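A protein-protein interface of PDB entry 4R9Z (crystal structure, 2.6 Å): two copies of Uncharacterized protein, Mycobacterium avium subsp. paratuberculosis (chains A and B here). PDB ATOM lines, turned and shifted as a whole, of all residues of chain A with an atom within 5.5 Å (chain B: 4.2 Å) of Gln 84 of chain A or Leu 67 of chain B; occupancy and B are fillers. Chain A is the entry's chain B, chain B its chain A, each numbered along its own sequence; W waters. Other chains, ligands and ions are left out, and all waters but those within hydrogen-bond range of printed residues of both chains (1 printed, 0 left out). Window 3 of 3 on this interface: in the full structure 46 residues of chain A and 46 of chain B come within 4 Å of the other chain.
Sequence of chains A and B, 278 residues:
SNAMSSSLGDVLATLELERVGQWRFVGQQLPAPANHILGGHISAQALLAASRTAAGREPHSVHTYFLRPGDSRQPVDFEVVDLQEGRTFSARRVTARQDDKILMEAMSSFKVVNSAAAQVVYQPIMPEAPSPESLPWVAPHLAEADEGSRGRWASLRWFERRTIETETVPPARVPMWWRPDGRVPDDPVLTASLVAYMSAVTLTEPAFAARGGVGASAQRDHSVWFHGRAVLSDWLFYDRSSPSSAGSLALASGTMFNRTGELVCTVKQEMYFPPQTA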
ATOM      1  N   ASP A  82     -16.280  21.576 -18.759  1.00  0.00           N
ATOM      2  CA  ASP A  82     -15.877  21.672 -20.157  1.00  0.00           C
ATOM      3  C   ASP A  82     -17.032  21.286 -21.091  1.00  0.00           C
ATOM      4  O   ASP A  82     -17.341  20.110 -21.253  1.00  0.00           O
ATOM      5  CB  ASP A  82     -14.650  20.780 -20.400  1.00  0.00           C
ATOM      6  CG  ASP A  82     -14.215  20.738 -21.859  1.00  0.00           C
ATOM      7  OD1 ASP A  82     -14.599  21.629 -22.642  1.00  0.00           O
ATOM      8  OD2 ASP A  82     -13.465  19.810 -22.222  1.00  0.00           O
ATOM      9  N   LEU A  83     -17.682  22.290 -21.673  1.00  0.00           N
ATOM     10  CA  LEU A  83     -18.775  22.091 -22.624  1.00  0.00           C
ATOM     11  C   LEU A  83     -18.252  21.794 -24.016  1.00  0.00           C
ATOM     12  O   LEU A  83     -18.839  21.012 -24.763  1.00  0.00           O
ATOM     13  CB  LEU A  83     -19.689  23.315 -22.669  1.00  0.00           C
ATOM     14  CG  LEU A  83     -20.314  23.704 -21.331  1.00  0.00           C
ATOM     15  CD1 LEU A  83     -21.222  24.907 -21.508  1.00  0.00           C
ATOM     16  CD2 LEU A  83     -21.068  22.526 -20.737  1.00  0.00           C
ATOM     17  N   GLN A  84     -17.164  22.461 -24.379  1.00  0.00           N
ATOM     18  CA  GLN A  84     -16.538  22.207 -25.658  1.00  0.00           C
ATOM     19  C   GLN A  84     -15.075  22.609 -25.673  1.00  0.00           C
ATOM     20  O   GLN A  84     -14.697  23.655 -25.155  1.00  0.00           O
ATOM     21  CB  GLN A  84     -17.276  22.957 -26.763  1.00  0.00           C
ATOM     22  CG  GLN A  84     -16.698  22.710 -28.141  1.00  0.00           C
ATOM     23  CD  GLN A  84     -16.772  23.926 -29.026  1.00  0.00           C
ATOM     24  OE1 GLN A  84     -16.672  25.058 -28.553  1.00  0.00           O
ATOM     25  NE2 GLN A  84     -16.948  23.704 -30.322  1.00  0.00           N
ATOM     26  N   GLU A  85     -14.253  21.773 -26.288  1.00  0.00           N
ATOM     27  CA  GLU A  85     -12.850  22.088 -26.441  1.00  0.00           C
ATOM     28  C   GLU A  85     -12.452  21.753 -27.860  1.00  0.00           C
ATOM     29  O   GLU A  85     -12.144  20.606 -28.177  1.00  0.00           O
ATOM     30  CB  GLU A  85     -11.997  21.323 -25.426  1.00  0.00           C
ATOM     31  CG  GLU A  85     -10.540  21.759 -25.394  1.00  0.00           C
ATOM     32  CD  GLU A  85     -10.366  23.202 -24.942  1.00  0.00           C
ATOM     33  OE1 GLU A  85     -11.236  23.715 -24.204  1.00  0.00           O
ATOM     34  OE2 GLU A  85      -9.354  23.825 -25.320  1.00  0.00           O
ATOM     35  N   GLY A  86     -12.483  22.762 -28.717  1.00  0.00           N
ATOM     36  CA  GLY A  86     -12.232  22.568 -30.129  1.00  0.00           C
ATOM     37  C   GLY A  86     -10.975  23.253 -30.615  1.00  0.00           C
ATOM     38  O   GLY A  86     -10.289  23.953 -29.864  1.00  0.00           O
ATOM     39  N   PHE A  89     -12.815  26.990 -30.972  1.00  0.00           N
ATOM     40  CA  PHE A  89     -13.640  27.460 -29.866  1.00  0.00           C
ATOM     41  C   PHE A  89     -13.519  26.637 -28.590  1.00  0.00           C
ATOM     42  O   PHE A  89     -13.240  25.438 -28.616  1.00  0.00           O
ATOM     43  CB  PHE A  89     -15.114  27.482 -30.286  1.00  0.00           C
ATOM     44  CG  PHE A  89     -15.477  28.626 -31.182  1.00  0.00           C
ATOM     45  CD1 PHE A  89     -15.735  29.880 -30.655  1.00  0.00           C
ATOM     46  CD2 PHE A  89     -15.570  28.444 -32.554  1.00  0.00           C
ATOM     47  CE1 PHE A  89     -16.073  30.938 -31.478  1.00  0.00           C
ATOM     48  CE2 PHE A  89     -15.904  29.494 -33.384  1.00  0.00           C
ATOM     49  CZ  PHE A  89     -16.156  30.745 -32.845  1.00  0.00           C
ATOM     50  N   SER A  90     -13.776  27.303 -27.474  1.00  0.00           N
ATOM     51  CA  SER A  90     -13.953  26.644 -26.193  1.00  0.00           C
ATOM     52  C   SER A  90     -15.259  27.120 -25.565  1.00  0.00           C
ATOM     53  O   SER A  90     -15.687  28.254 -25.781  1.00  0.00           O
ATOM     54  CB  SER A  90     -12.774  26.937 -25.260  1.00  0.00           C
ATOM     55  OG  SER A  90     -11.574  26.377 -25.757  1.00  0.00           O
ATOM     56  N   ALA A  91     -15.891  26.247 -24.791  1.00  0.00           N
ATOM     57  CA  ALA A  91     -17.098  26.609 -24.067  1.00  0.00           C
ATOM     58  C   ALA A  91     -17.011  26.092 -22.641  1.00  0.00           C
ATOM     59  O   ALA A  91     -16.499  24.999 -22.400  1.00  0.00           O
ATOM     60  CB  ALA A  91     -18.323  26.057 -24.762  1.00  0.00           C
ATOM     61  N   ARG A  92     -17.492  26.890 -21.696  1.00  0.00           N
ATOM     62  CA  ARG A  92     -17.468  26.505 -20.288  1.00  0.00           C
ATOM     63  C   ARG A  92     -18.802  26.743 -19.602  1.00  0.00           C
ATOM     64  O   ARG A  92     -19.543  27.652 -19.964  1.00  0.00           O
ATOM     65  CB  ARG A  92     -16.366  27.259 -19.538  1.00  0.00           C
ATOM     66  CG  ARG A  92     -14.976  27.028 -20.098  1.00  0.00           C
ATOM     67  CD  ARG A  92     -14.540  25.592 -19.878  1.00  0.00           C
ATOM     68  NE  ARG A  92     -13.162  25.374 -20.302  1.00  0.00           N
ATOM     69  CZ  ARG A  92     -12.831  24.738 -21.419  1.00  0.00           C
ATOM     70  NH1 ARG A  92     -13.779  24.263 -22.208  1.00  0.00           N
ATOM     71  NH2 ARG A  92     -11.557  24.578 -21.746  1.00  0.00           N
ATOM     72  N   TYR B  65     -26.199  28.174 -26.155  1.00  0.00           N
ATOM     73  CA  TYR B  65     -24.950  28.082 -26.909  1.00  0.00           C
ATOM     74  C   TYR B  65     -25.013  26.909 -27.875  1.00  0.00           C
ATOM     75  O   TYR B  65     -25.382  25.810 -27.484  1.00  0.00           O
ATOM     76  CB  TYR B  65     -23.755  27.907 -25.979  1.00  0.00           C
ATOM     77  CG  TYR B  65     -23.091  29.199 -25.584  1.00  0.00           C
ATOM     78  CD1 TYR B  65     -22.450  29.995 -26.527  1.00  0.00           C
ATOM     79  CD2 TYR B  65     -23.097  29.619 -24.268  1.00  0.00           C
ATOM     80  CE1 TYR B  65     -21.844  31.181 -26.163  1.00  0.00           C
ATOM     81  CE2 TYR B  65     -22.492  30.798 -23.894  1.00  0.00           C
ATOM     82  CZ  TYR B  65     -21.867  31.576 -24.842  1.00  0.00           C
ATOM     83  OH  TYR B  65     -21.266  32.749 -24.458  1.00  0.00           O
ATOM     84  N   PHE B  66     -24.665  27.138 -29.135  1.00  0.00           N
ATOM     85  CA  PHE B  66     -24.573  26.042 -30.098  1.00  0.00           C
ATOM     86  C   PHE B  66     -23.119  25.636 -30.260  1.00  0.00           C
ATOM     87  O   PHE B  66     -22.305  26.411 -30.757  1.00  0.00           O
ATOM     88  CB  PHE B  66     -25.193  26.444 -31.436  1.00  0.00           C
ATOM     89  CG  PHE B  66     -26.587  26.969 -31.302  1.00  0.00           C
ATOM     90  CD1 PHE B  66     -27.631  26.116 -30.982  1.00  0.00           C
ATOM     91  CD2 PHE B  66     -26.853  28.315 -31.458  1.00  0.00           C
ATOM     92  CE1 PHE B  66     -28.912  26.593 -30.841  1.00  0.00           C
ATOM     93  CE2 PHE B  66     -28.134  28.797 -31.322  1.00  0.00           C
ATOM     94  CZ  PHE B  66     -29.165  27.936 -31.013  1.00  0.00           C
ATOM     95  N   LEU B  67     -22.804  24.414 -29.841  1.00  0.00           N
ATOM     96  CA  LEU B  67     -21.418  24.010 -29.631  1.00  0.00           C
ATOM     97  C   LEU B  67     -20.872  23.096 -30.717  1.00  0.00           C
ATOM     98  O   LEU B  67     -19.741  23.262 -31.167  1.00  0.00           O
ATOM     99  CB  LEU B  67     -21.291  23.325 -28.276  1.00  0.00           C
ATOM    100  CG  LEU B  67     -21.790  24.186 -27.119  1.00  0.00           C
ATOM    101  CD1 LEU B  67     -21.727  23.429 -25.805  1.00  0.00           C
ATOM    102  CD2 LEU B  67     -20.983  25.468 -27.055  1.00  0.00           C
ATOM    103  N   ARG B  68     -21.669  22.116 -31.118  1.00  0.00           N
ATOM    104  CA  ARG B  68     -21.249  21.157 -32.128  1.00  0.00           C
ATOM    105  C   ARG B  68     -22.407  20.951 -33.085  1.00  0.00           C
ATOM    106  O   ARG B  68     -23.561  20.958 -32.665  1.00  0.00           O
ATOM    107  CB  ARG B  68     -20.829  19.824 -31.497  1.00  0.00           C
ATOM    108  CG  ARG B  68     -19.675  19.909 -30.504  1.00  0.00           C
ATOM    109  CD  ARG B  68     -18.316  19.926 -31.193  1.00  0.00           C
ATOM    110  NE  ARG B  68     -18.072  18.702 -31.951  1.00  0.00           N
ATOM    111  CZ  ARG B  68     -17.632  17.567 -31.417  1.00  0.00           C
ATOM    112  NH1 ARG B  68     -17.385  17.492 -30.118  1.00  0.00           N
ATOM    113  NH2 ARG B  68     -17.442  16.501 -32.182  1.00  0.00           N
ATOM    114  N   ILE B 102     -21.801  16.668 -27.040  1.00  0.00           N
ATOM    115  CA  ILE B 102     -22.617  17.813 -26.622  1.00  0.00           C
ATOM    116  C   ILE B 102     -22.837  18.811 -27.754  1.00  0.00           C
ATOM    117  O   ILE B 102     -21.893  19.453 -28.221  1.00  0.00           O
ATOM    118  CB  ILE B 102     -21.982  18.550 -25.434  1.00  0.00           C
ATOM    119  CG1 ILE B 102     -21.876  17.618 -24.227  1.00  0.00           C
ATOM    120  CG2 ILE B 102     -22.800  19.775 -25.074  1.00  0.00           C
ATOM    121  CD1 ILE B 102     -21.113  18.220 -23.060  1.00  0.00           C
ATOM    122  N   LEU B 103     -24.096  18.967 -28.157  1.00  0.00           N
ATOM    123  CA  LEU B 103     -24.453  19.792 -29.307  1.00  0.00           C
ATOM    124  C   LEU B 103     -24.747  21.232 -28.901  1.00  0.00           C
ATOM    125  O   LEU B 103     -24.269  22.185 -29.524  1.00  0.00           O
ATOM    126  CB  LEU B 103     -25.670  19.192 -30.011  1.00  0.00           C
ATOM    127  CG  LEU B 103     -25.612  17.704 -30.375  1.00  0.00           C
ATOM    128  CD1 LEU B 103     -26.947  17.264 -30.936  1.00  0.00           C
ATOM    129  CD2 LEU B 103     -24.497  17.418 -31.373  1.00  0.00           C
ATOM    130  N   ARG B 220     -23.527  30.641 -33.068  1.00  0.00           N
ATOM    131  CA  ARG B 220     -22.865  30.300 -31.834  1.00  0.00           C
ATOM    132  C   ARG B 220     -23.737  30.407 -30.580  1.00  0.00           C
ATOM    133  O   ARG B 220     -23.782  29.568 -29.754  1.00  0.00           O
ATOM    134  CB  ARG B 220     -21.598  31.095 -31.698  1.00  0.00           C
ATOM    135  CG  ARG B 220     -20.796  30.714 -30.496  1.00  0.00           C
ATOM    136  CD  ARG B 220     -20.356  29.285 -30.490  1.00  0.00           C
ATOM    137  NE  ARG B 220     -19.364  29.132 -29.477  1.00  0.00           N
ATOM    138  CZ  ARG B 220     -18.678  28.046 -29.268  1.00  0.00           C
ATOM    139  NH1 ARG B 220     -18.852  26.998 -30.007  1.00  0.00           N
ATOM    140  NH2 ARG B 220     -17.805  28.033 -28.316  1.00  0.00           N
HETATM  141  O   HOH W   1     -19.219  20.032 -27.299  1.00  0.00           O
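No position is printed for both chains.
Of the 7 pairs that touch across the chains among the printed residues, none has its exchanged pair printed and touching as well.
Printed residues of chain B within 4 Å of Gln 84 of chain A: Leu 67 (3.0 Å) and Arg 220 (3.2 Å).
Of chain A, only Leu 83 (3.7 Å), Gln 84 (3.0 Å) and Ala 91 (3.6 Å) come within 4 Å of Leu 67 of chain B.
Of the printed residues of chain A, Ile 102 of chain B touches Leu 83.
Of the printed residues of chain B, Leu 83 of chain A touches Leu 67 and Ile 102.
Printed residues of chain B within 4 Å of Ala 91 of chain A: Leu 67 (3.6 Å).
Glu 85 of chain A touches none of the printed residues of chain B.
Gly 86 of chain A touches none of the printed residues of chain B.
The nearest residue of chain B that does not touch Gln 84 of chain A is Arg 68 of chain B (4.1 Å).
The nearest printed residue of chain A that does not touch Leu 67 of chain B is Ser 90 of chain A (6.1 Å).
Among the printed residues, pairs that only touch across the chains: Phe 89 of chain A with Arg 220 of chain B, Ala 91 of chain A with Leu 67 of chain B, Leu 83 of chain A with Leu 67 of chain B and Leu 83 of chain A with Ile 102 of chain B.
Water W1 lies within hydrogen-bond range of O of Leu 83 of chain A and O of Ile 102 of chain B.
Printed residues of chain A that touch a printed residue of chain B: Leu 83, Gln 84, Phe 89, Ser 90 and Ala 91.
Hydrophobic or aromatic side chains of chain A that line the printed part of chain B: Leu 83, Phe 89 and Ala 91.
Along chain A the printed residues that touch a printed residue of chain B span positions 83 to 91.
Printed residues of chain B that touch a printed residue of chain A: Leu 67, Ile 102 and Arg 220.
Hydrophobic or aromatic side chains of chain B that line the printed part of chain A: Leu 67 and Ile 102.
Among the printed residues, 7 pairs touch across the chains.
Among the printed residues, no Asp or Glu carboxylate lies within 4 Å of a Lys or Arg side-chain nitrogen of the other chain.
NH2 of Arg 220 of chain B sits at hydrogen-bond distance from OE1 of Gln 84 of chain A (3.2 Å).
The backbone carbonyl oxygen of Ser 90 of chain A sits at hydrogen-bond distance from the guanidinium group of Arg 220 of chain B (3.3 Å).
O of Leu 67 of chain B is in hydrogen-bond range of NE2 of Gln 84 of chain A (3.0 Å).
The backbone NH (N) of Leu 67 of chain B is in hydrogen-bond range of the backbone carbonyl oxygen (O) of Leu 103 of chain B.
OD1 of Asp 82 of chain A sits at hydrogen-bond distance from N of Gln 84 of chain A (3.2 Å).
The backbone carbonyl oxygen (O) of Gln 84 of chain A lies within hydrogen-bond range of the backbone NH (N) of Ala 91 of chain A (2.9 Å).
O of Ala 91 of chain A sits at hydrogen-bond distance from N of Leu 83 of chain A, at 3.0 Å.
O of Phe 89 of chain A sits close to OE1 of Gln 84 of chain A.
OE1 of Glu 85 of chain A is in hydrogen-bond range of OG of Ser 90 of chain A (3.1 Å).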
